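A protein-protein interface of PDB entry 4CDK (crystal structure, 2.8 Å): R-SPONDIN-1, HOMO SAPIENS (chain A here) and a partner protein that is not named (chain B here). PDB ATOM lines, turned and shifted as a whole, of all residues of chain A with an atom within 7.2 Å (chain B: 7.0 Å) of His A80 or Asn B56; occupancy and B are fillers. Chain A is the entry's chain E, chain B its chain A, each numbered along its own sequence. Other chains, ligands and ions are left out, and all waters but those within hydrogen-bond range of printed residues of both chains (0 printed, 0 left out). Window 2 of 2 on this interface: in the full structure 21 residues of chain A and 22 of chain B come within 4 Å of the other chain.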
ATOM      1  N   PHE A  56      -6.996 -10.923 -10.215  1.00  0.00           N
ATOM      2  CA  PHE A  56      -6.447 -11.829  -9.226  1.00  0.00           C
ATOM      3  C   PHE A  56      -7.014 -11.617  -7.824  1.00  0.00           C
ATOM      4  O   PHE A  56      -7.626 -10.580  -7.500  1.00  0.00           O
ATOM      5  CB  PHE A  56      -4.913 -11.742  -9.197  1.00  0.00           C
ATOM      6  CG  PHE A  56      -4.375 -10.391  -8.832  1.00  0.00           C
ATOM      7  CD1 PHE A  56      -4.223  -9.407  -9.795  1.00  0.00           C
ATOM      8  CD2 PHE A  56      -3.997 -10.110  -7.531  1.00  0.00           C
ATOM      9  CE1 PHE A  56      -3.716  -8.166  -9.467  1.00  0.00           C
ATOM     10  CE2 PHE A  56      -3.491  -8.870  -7.196  1.00  0.00           C
ATOM     11  CZ  PHE A  56      -3.353  -7.897  -8.167  1.00  0.00           C
ATOM     12  N   ALA A  58      -6.743 -10.770  -4.566  1.00  0.00           N
ATOM     13  CA  ALA A  58      -5.989  -9.987  -3.590  1.00  0.00           C
ATOM     14  C   ALA A  58      -6.600 -10.153  -2.198  1.00  0.00           C
ATOM     15  O   ALA A  58      -7.563  -9.486  -1.821  1.00  0.00           O
ATOM     16  CB  ALA A  58      -5.961  -8.534  -3.982  1.00  0.00           C
ATOM     17  N   ILE A  67      -8.567  -7.816  -8.238  1.00  0.00           N
ATOM     18  CA  ILE A  67      -7.846  -6.709  -8.860  1.00  0.00           C
ATOM     19  C   ILE A  67      -7.387  -7.039 -10.268  1.00  0.00           C
ATOM     20  O   ILE A  67      -6.851  -8.107 -10.509  1.00  0.00           O
ATOM     21  CB  ILE A  67      -6.628  -6.272  -8.018  1.00  0.00           C
ATOM     22  CG1 ILE A  67      -7.092  -5.680  -6.690  1.00  0.00           C
ATOM     23  CG2 ILE A  67      -5.806  -5.223  -8.753  1.00  0.00           C
ATOM     24  CD1 ILE A  67      -5.985  -5.507  -5.689  1.00  0.00           C
ATOM     25  N   LYS A  68      -7.595  -6.111 -11.194  1.00  0.00           N
ATOM     26  CA  LYS A  68      -7.216  -6.325 -12.585  1.00  0.00           C
ATOM     27  C   LYS A  68      -5.724  -6.513 -12.733  1.00  0.00           C
ATOM     28  O   LYS A  68      -4.946  -5.727 -12.201  1.00  0.00           O
ATOM     29  CB  LYS A  68      -7.644  -5.155 -13.474  1.00  0.00           C
ATOM     30  CG  LYS A  68      -7.204  -5.344 -14.920  1.00  0.00           C
ATOM     31  CD  LYS A  68      -8.004  -6.398 -15.659  1.00  0.00           C
ATOM     32  CE  LYS A  68      -7.465  -6.536 -17.068  1.00  0.00           C
ATOM     33  NZ  LYS A  68      -7.894  -7.818 -17.675  1.00  0.00           N
ATOM     34  N   CYS A  69      -5.324  -7.536 -13.483  1.00  0.00           N
ATOM     35  CA  CYS A  69      -3.913  -7.740 -13.741  1.00  0.00           C
ATOM     36  C   CYS A  69      -3.554  -6.813 -14.900  1.00  0.00           C
ATOM     37  O   CYS A  69      -4.348  -6.614 -15.821  1.00  0.00           O
ATOM     38  CB  CYS A  69      -3.628  -9.209 -14.083  1.00  0.00           C
ATOM     39  SG  CYS A  69      -1.886  -9.691 -14.131  1.00  0.00           S
ATOM     40  N   LYS A  70      -2.352  -6.254 -14.854  1.00  0.00           N
ATOM     41  CA  LYS A  70      -1.937  -5.268 -15.841  1.00  0.00           C
ATOM     42  C   LYS A  70      -0.826  -5.811 -16.724  1.00  0.00           C
ATOM     43  O   LYS A  70      -0.345  -5.133 -17.627  1.00  0.00           O
ATOM     44  CB  LYS A  70      -1.508  -3.978 -15.146  1.00  0.00           C
ATOM     45  CG  LYS A  70      -2.623  -3.372 -14.315  1.00  0.00           C
ATOM     46  CD  LYS A  70      -3.737  -2.836 -15.197  1.00  0.00           C
ATOM     47  CE  LYS A  70      -3.269  -1.636 -16.000  1.00  0.00           C
ATOM     48  NZ  LYS A  70      -2.700  -0.574 -15.125  1.00  0.00           N
ATOM     49  N   ILE A  71      -0.442  -7.054 -16.476  1.00  0.00           N
ATOM     50  CA  ILE A  71       0.653  -7.649 -17.210  1.00  0.00           C
ATOM     51  C   ILE A  71       0.061  -8.331 -18.418  1.00  0.00           C
ATOM     52  O   ILE A  71      -1.028  -8.906 -18.363  1.00  0.00           O
ATOM     53  CB  ILE A  71       1.453  -8.652 -16.360  1.00  0.00           C
ATOM     54  CG1 ILE A  71       1.993  -7.949 -15.130  1.00  0.00           C
ATOM     55  CG2 ILE A  71       2.689  -9.116 -17.111  1.00  0.00           C
ATOM     56  CD1 ILE A  71       2.883  -6.784 -15.494  1.00  0.00           C
ATOM     57  N   GLU A  72       0.801  -8.281 -19.512  1.00  0.00           N
ATOM     58  CA  GLU A  72       0.257  -8.686 -20.782  1.00  0.00           C
ATOM     59  C   GLU A  72       0.804 -10.060 -21.087  1.00  0.00           C
ATOM     60  O   GLU A  72       1.976 -10.351 -20.832  1.00  0.00           O
ATOM     61  CB  GLU A  72       0.620  -7.677 -21.873  1.00  0.00           C
ATOM     62  CG  GLU A  72      -0.047  -7.928 -23.210  1.00  0.00           C
ATOM     63  CD  GLU A  72       0.241  -6.828 -24.212  1.00  0.00           C
ATOM     64  OE1 GLU A  72       0.948  -5.860 -23.852  1.00  0.00           O
ATOM     65  OE2 GLU A  72      -0.245  -6.929 -25.360  1.00  0.00           O
ATOM     66  N   CYS A  77      -1.365 -13.545 -12.004  1.00  0.00           N
ATOM     67  CA  CYS A  77      -0.335 -12.649 -11.499  1.00  0.00           C
ATOM     68  C   CYS A  77      -0.434 -12.464  -9.993  1.00  0.00           C
ATOM     69  O   CYS A  77      -1.523 -12.447  -9.426  1.00  0.00           O
ATOM     70  CB  CYS A  77      -0.395 -11.292 -12.204  1.00  0.00           C
ATOM     71  SG  CYS A  77      -2.000 -10.481 -12.259  1.00  0.00           S
ATOM     72  N   PHE A  78       0.723 -12.316  -9.360  1.00  0.00           N
ATOM     73  CA  PHE A  78       0.820 -12.182  -7.914  1.00  0.00           C
ATOM     74  C   PHE A  78       0.325 -10.806  -7.483  1.00  0.00           C
ATOM     75  O   PHE A  78      -0.295 -10.654  -6.434  1.00  0.00           O
ATOM     76  CB  PHE A  78       2.258 -12.387  -7.449  1.00  0.00           C
ATOM     77  CG  PHE A  78       2.434 -12.261  -5.972  1.00  0.00           C
ATOM     78  CD1 PHE A  78       2.102 -13.317  -5.141  1.00  0.00           C
ATOM     79  CD2 PHE A  78       2.906 -11.089  -5.407  1.00  0.00           C
ATOM     80  CE1 PHE A  78       2.250 -13.215  -3.773  1.00  0.00           C
ATOM     81  CE2 PHE A  78       3.052 -10.981  -4.038  1.00  0.00           C
ATOM     82  CZ  PHE A  78       2.726 -12.045  -3.223  1.00  0.00           C
ATOM     83  N   SER A  79       0.609  -9.806  -8.308  1.00  0.00           N
ATOM     84  CA  SER A  79       0.135  -8.447  -8.082  1.00  0.00           C
ATOM     85  C   SER A  79      -0.186  -7.848  -9.442  1.00  0.00           C
ATOM     86  O   SER A  79      -0.105  -8.543 -10.453  1.00  0.00           O
ATOM     87  CB  SER A  79       1.167  -7.606  -7.332  1.00  0.00           C
ATOM     88  OG  SER A  79       2.453  -7.751  -7.899  1.00  0.00           O
ATOM     89  N   HIS A  80      -0.533  -6.566  -9.486  1.00  0.00           N
ATOM     90  CA  HIS A  80      -0.953  -5.971 -10.748  1.00  0.00           C
ATOM     91  C   HIS A  80       0.203  -5.853 -11.734  1.00  0.00           C
ATOM     92  O   HIS A  80      -0.014  -5.919 -12.946  1.00  0.00           O
ATOM     93  CB  HIS A  80      -1.596  -4.597 -10.525  1.00  0.00           C
ATOM     94  CG  HIS A  80      -0.697  -3.600  -9.865  1.00  0.00           C
ATOM     95  ND1 HIS A  80      -0.335  -3.686  -8.538  1.00  0.00           N
ATOM     96  CD2 HIS A  80      -0.096  -2.487 -10.347  1.00  0.00           C
ATOM     97  CE1 HIS A  80       0.454  -2.671  -8.231  1.00  0.00           C
ATOM     98  NE2 HIS A  80       0.615  -1.929  -9.312  1.00  0.00           N
ATOM     99  N   ASN A  81       1.427  -5.697 -11.238  1.00  0.00           N
ATOM    100  CA  ASN A  81       2.560  -5.647 -12.153  1.00  0.00           C
ATOM    101  C   ASN A  81       3.579  -6.779 -12.015  1.00  0.00           C
ATOM    102  O   ASN A  81       4.499  -6.875 -12.827  1.00  0.00           O
ATOM    103  CB  ASN A  81       3.275  -4.304 -12.014  1.00  0.00           C
ATOM    104  CG  ASN A  81       2.520  -3.172 -12.685  1.00  0.00           C
ATOM    105  OD1 ASN A  81       1.751  -3.394 -13.621  1.00  0.00           O
ATOM    106  ND2 ASN A  81       2.735  -1.950 -12.210  1.00  0.00           N
ATOM    107  N   PHE A  82       3.461  -7.620 -10.991  1.00  0.00           N
ATOM    108  CA  PHE A  82       4.307  -8.809 -10.953  1.00  0.00           C
ATOM    109  C   PHE A  82       3.475 -10.024 -11.377  1.00  0.00           C
ATOM    110  O   PHE A  82       2.309 -10.139 -11.003  1.00  0.00           O
ATOM    111  CB  PHE A  82       4.938  -9.019  -9.581  1.00  0.00           C
ATOM    112  CG  PHE A  82       6.179  -9.862  -9.622  1.00  0.00           C
ATOM    113  CD1 PHE A  82       6.109 -11.245  -9.574  1.00  0.00           C
ATOM    114  CD2 PHE A  82       7.426  -9.264  -9.738  1.00  0.00           C
ATOM    115  CE1 PHE A  82       7.261 -12.017  -9.625  1.00  0.00           C
ATOM    116  CE2 PHE A  82       8.579 -10.024  -9.787  1.00  0.00           C
ATOM    117  CZ  PHE A  82       8.498 -11.403  -9.733  1.00  0.00           C
ATOM    118  N   CYS A  83       4.075 -10.939 -12.132  1.00  0.00           N
ATOM    119  CA  CYS A  83       3.367 -12.123 -12.615  1.00  0.00           C
ATOM    120  C   CYS A  83       4.017 -13.412 -12.107  1.00  0.00           C
ATOM    121  O   CYS A  83       5.241 -13.516 -12.063  1.00  0.00           O
ATOM    122  CB  CYS A  83       3.321 -12.108 -14.148  1.00  0.00           C
ATOM    123  SG  CYS A  83       2.127 -13.224 -14.919  1.00  0.00           S
ATOM    124  N   GLY A  95       8.903 -10.830 -13.346  1.00  0.00           N
ATOM    125  CA  GLY A  95       7.501 -10.519 -13.162  1.00  0.00           C
ATOM    126  C   GLY A  95       6.724 -10.247 -14.435  1.00  0.00           C
ATOM    127  O   GLY A  95       5.536  -9.948 -14.375  1.00  0.00           O
ATOM    128  N   ARG A  96       7.385 -10.322 -15.587  1.00  0.00           N
ATOM    129  CA  ARG A  96       6.728  -9.976 -16.845  1.00  0.00           C
ATOM    130  C   ARG A  96       6.845 -11.091 -17.882  1.00  0.00           C
ATOM    131  O   ARG A  96       7.758 -11.915 -17.832  1.00  0.00           O
ATOM    132  CB  ARG A  96       7.313  -8.680 -17.410  1.00  0.00           C
ATOM    133  CG  ARG A  96       6.992  -7.463 -16.571  1.00  0.00           C
ATOM    134  CD  ARG A  96       7.564  -6.192 -17.167  1.00  0.00           C
ATOM    135  NE  ARG A  96       7.119  -5.020 -16.418  1.00  0.00           N
ATOM    136  CZ  ARG A  96       5.933  -4.440 -16.566  1.00  0.00           C
ATOM    137  NH1 ARG A  96       5.061  -4.918 -17.443  1.00  0.00           N
ATOM    138  NH2 ARG A  96       5.619  -3.380 -15.833  1.00  0.00           N
ATOM    139  N   LEU B  53     -10.144   4.718  -5.870  1.00  0.00           N
ATOM    140  CA  LEU B  53      -8.937   5.529  -5.759  1.00  0.00           C
ATOM    141  C   LEU B  53      -7.987   4.978  -4.697  1.00  0.00           C
ATOM    142  O   LEU B  53      -7.069   5.665  -4.251  1.00  0.00           O
ATOM    143  CB  LEU B  53      -9.297   6.985  -5.451  1.00  0.00           C
ATOM    144  CG  LEU B  53     -10.069   7.717  -6.554  1.00  0.00           C
ATOM    145  CD1 LEU B  53     -10.843   8.898  -5.990  1.00  0.00           C
ATOM    146  CD2 LEU B  53      -9.126   8.172  -7.657  1.00  0.00           C
ATOM    147  N   CYS B  54      -8.219   3.732  -4.296  1.00  0.00           N
ATOM    148  CA  CYS B  54      -7.426   3.091  -3.251  1.00  0.00           C
ATOM    149  C   CYS B  54      -6.162   2.427  -3.791  1.00  0.00           C
ATOM    150  O   CYS B  54      -5.934   2.385  -5.000  1.00  0.00           O
ATOM    151  CB  CYS B  54      -8.270   2.054  -2.510  1.00  0.00           C
ATOM    152  SG  CYS B  54      -9.620   2.749  -1.532  1.00  0.00           S
ATOM    153  N   ASN B  55      -5.352   1.906  -2.872  1.00  0.00           N
ATOM    154  CA  ASN B  55      -4.090   1.244  -3.198  1.00  0.00           C
ATOM    155  C   ASN B  55      -4.252   0.040  -4.120  1.00  0.00           C
ATOM    156  O   ASN B  55      -5.110  -0.815  -3.894  1.00  0.00           O
ATOM    157  CB  ASN B  55      -3.376   0.813  -1.916  1.00  0.00           C
ATOM    158  CG  ASN B  55      -2.913   1.992  -1.084  1.00  0.00           C
ATOM    159  OD1 ASN B  55      -2.583   3.052  -1.618  1.00  0.00           O
ATOM    160  ND2 ASN B  55      -2.886   1.813   0.231  1.00  0.00           N
ATOM    161  N   ASN B  56      -3.444   0.028  -5.179  1.00  0.00           N
ATOM    162  CA  ASN B  56      -3.343  -1.065  -6.153  1.00  0.00           C
ATOM    163  C   ASN B  56      -4.560  -1.076  -7.089  1.00  0.00           C
ATOM    164  O   ASN B  56      -4.426  -1.382  -8.274  1.00  0.00           O
ATOM    165  CB  ASN B  56      -3.162  -2.420  -5.440  1.00  0.00           C
ATOM    166  CG  ASN B  56      -2.779  -3.558  -6.391  1.00  0.00           C
ATOM    167  OD1 ASN B  56      -2.996  -3.490  -7.599  1.00  0.00           O
ATOM    168  ND2 ASN B  56      -2.186  -4.610  -5.834  1.00  0.00           N
ATOM    169  N   ASN B  57      -5.737  -0.707  -6.591  1.00  0.00           N
ATOM    170  CA  ASN B  57      -6.887  -0.561  -7.485  1.00  0.00           C
ATOM    171  C   ASN B  57      -6.702   0.601  -8.440  1.00  0.00           C
ATOM    172  O   ASN B  57      -7.158   0.544  -9.571  1.00  0.00           O
ATOM    173  CB  ASN B  57      -8.192  -0.381  -6.719  1.00  0.00           C
ATOM    174  CG  ASN B  57      -8.553  -1.599  -5.920  1.00  0.00           C
ATOM    175  OD1 ASN B  57      -8.687  -1.535  -4.697  1.00  0.00           O
ATOM    176  ND2 ASN B  57      -8.624  -2.741  -6.592  1.00  0.00           N
ATOM    177  N   ASP B  58      -6.085   1.673  -7.955  1.00  0.00           N
ATOM    178  CA  ASP B  58      -5.716   2.815  -8.790  1.00  0.00           C
ATOM    179  C   ASP B  58      -5.236   2.426 -10.189  1.00  0.00           C
ATOM    180  O   ASP B  58      -5.748   2.932 -11.188  1.00  0.00           O
ATOM    181  CB  ASP B  58      -4.650   3.652  -8.088  1.00  0.00           C
ATOM    182  CG  ASP B  58      -5.249   4.632  -7.107  1.00  0.00           C
ATOM    183  OD1 ASP B  58      -6.293   5.231  -7.443  1.00  0.00           O
ATOM    184  OD2 ASP B  58      -4.684   4.807  -6.008  1.00  0.00           O
ATOM    185  N   GLU B  59      -4.267   1.517 -10.260  1.00  0.00           N
ATOM    186  CA  GLU B  59      -3.750   1.056 -11.546  1.00  0.00           C
ATOM    187  C   GLU B  59      -4.658   0.017 -12.206  1.00  0.00           C
ATOM    188  O   GLU B  59      -4.173  -0.935 -12.813  1.00  0.00           O
ATOM    189  CB  GLU B  59      -2.350   0.457 -11.369  1.00  0.00           C
ATOM    190  CG  GLU B  59      -1.328   1.398 -10.736  1.00  0.00           C
ATOM    191  CD  GLU B  59      -1.224   1.224  -9.230  1.00  0.00           C
ATOM    192  OE1 GLU B  59      -2.054   0.486  -8.659  1.00  0.00           O
ATOM    193  OE2 GLU B  59      -0.311   1.819  -8.619  1.00  0.00           O
ATOM    194  N   GLU B  60      -5.968   0.195 -12.074  1.00  0.00           N
ATOM    195  CA  GLU B  60      -6.930  -0.759 -12.609  1.00  0.00           C
ATOM    196  C   GLU B  60      -6.923  -0.594 -14.125  1.00  0.00           C
ATOM    197  O   GLU B  60      -6.689  -1.531 -14.881  1.00  0.00           O
ATOM    198  CB  GLU B  60      -8.330  -0.493 -12.047  1.00  0.00           C
ATOM    199  CG  GLU B  60      -9.350  -1.596 -12.246  1.00  0.00           C
ATOM    200  CD  GLU B  60      -9.139  -2.728 -11.250  1.00  0.00           C
ATOM    201  OE1 GLU B  60      -8.190  -2.643 -10.440  1.00  0.00           O
ATOM    202  OE2 GLU B  60      -9.929  -3.695 -11.259  1.00  0.00           O
ATOM    203  N   ARG B  92      -5.054  11.787  -5.378  1.00  0.00           N
ATOM    204  CA  ARG B  92      -4.830  10.568  -6.135  1.00  0.00           C
ATOM    205  C   ARG B  92      -5.388  10.706  -7.544  1.00  0.00           C
ATOM    206  O   ARG B  92      -4.728  10.345  -8.521  1.00  0.00           O
ATOM    207  CB  ARG B  92      -5.461   9.367  -5.433  1.00  0.00           C
ATOM    208  CG  ARG B  92      -5.053   8.046  -6.040  1.00  0.00           C
ATOM    209  CD  ARG B  92      -3.557   7.831  -5.849  1.00  0.00           C
ATOM    210  NE  ARG B  92      -3.051   6.694  -6.612  1.00  0.00           N
ATOM    211  CZ  ARG B  92      -2.032   6.758  -7.462  1.00  0.00           C
ATOM    212  NH1 ARG B  92      -1.406   7.909  -7.664  1.00  0.00           N
ATOM    213  NH2 ARG B  92      -1.639   5.669  -8.112  1.00  0.00           N
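OD1 of Asn B56 sits at hydrogen-bond distance from ND1 of His A80 (2.8 Å).
The backbone carbonyl oxygen (O) of Glu B59 is in hydrogen-bond range of the side-chain amino group (NZ) of Lys A70, 2.8 Å away.
OE2 of Glu B60 sits at hydrogen-bond distance from N of Lys A68 (3.4 Å).
The backbone carbonyl oxygen (O) of Ile A67 is in hydrogen-bond range of the backbone NH (N) of Phe A56, at 2.8 Å.
O of His A80 lies within hydrogen-bond range of N of Lys A70 (3.0 Å).
The side-chain sulfur (SG) of Cys A69 is disulfide-bonded to the side-chain sulfur (SG) of Cys A77, at 2.0 Å.
Of the 17 printed residues of chain A, 4 touch a printed residue of chain B.
Printed residues of chain A that touch a printed residue of chain B: Ile A67, Lys A68, Lys A70 and His A80.
Printed residues of chain B that touch a printed residue of chain A: Asn B56, Asn B57, Glu B59 and Glu B60.
Among the printed residues, no Asp or Glu carboxylate lies within 4 Å of a Lys or Arg side-chain nitrogen of the other chain.
Among the printed residues, merely in contact across the chains: Lys A70 with Glu B60 (3.2 Å), Ile A67 with Asn B57 (3.3 Å), Ile A67 with Asn B56 (3.5 Å), His A80 with Glu B59 (3.7 Å) and Ile A67 with Glu B60 (3.9 Å).
Of chain A, only Ile A67 (3.5 Å) and His A80 (2.8 Å) come within 4 Å of Asn B56.
Of the printed residues of chain B, Lys A68 touches Glu B60 (3.4 Å).
Of the printed residues of chain A, Glu B60 touches Ile A67, Lys A68 and Lys A70.
Phe A82 touches none of the printed residues of chain B.
Ser A79 touches none of the printed residues of chain B.
The nearest residue of chain B that does not touch His A80 is Asn B57 (6.5 Å).
The nearest printed residue of chain A that does not touch Glu B60 is Cys A69 (5.7 Å).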
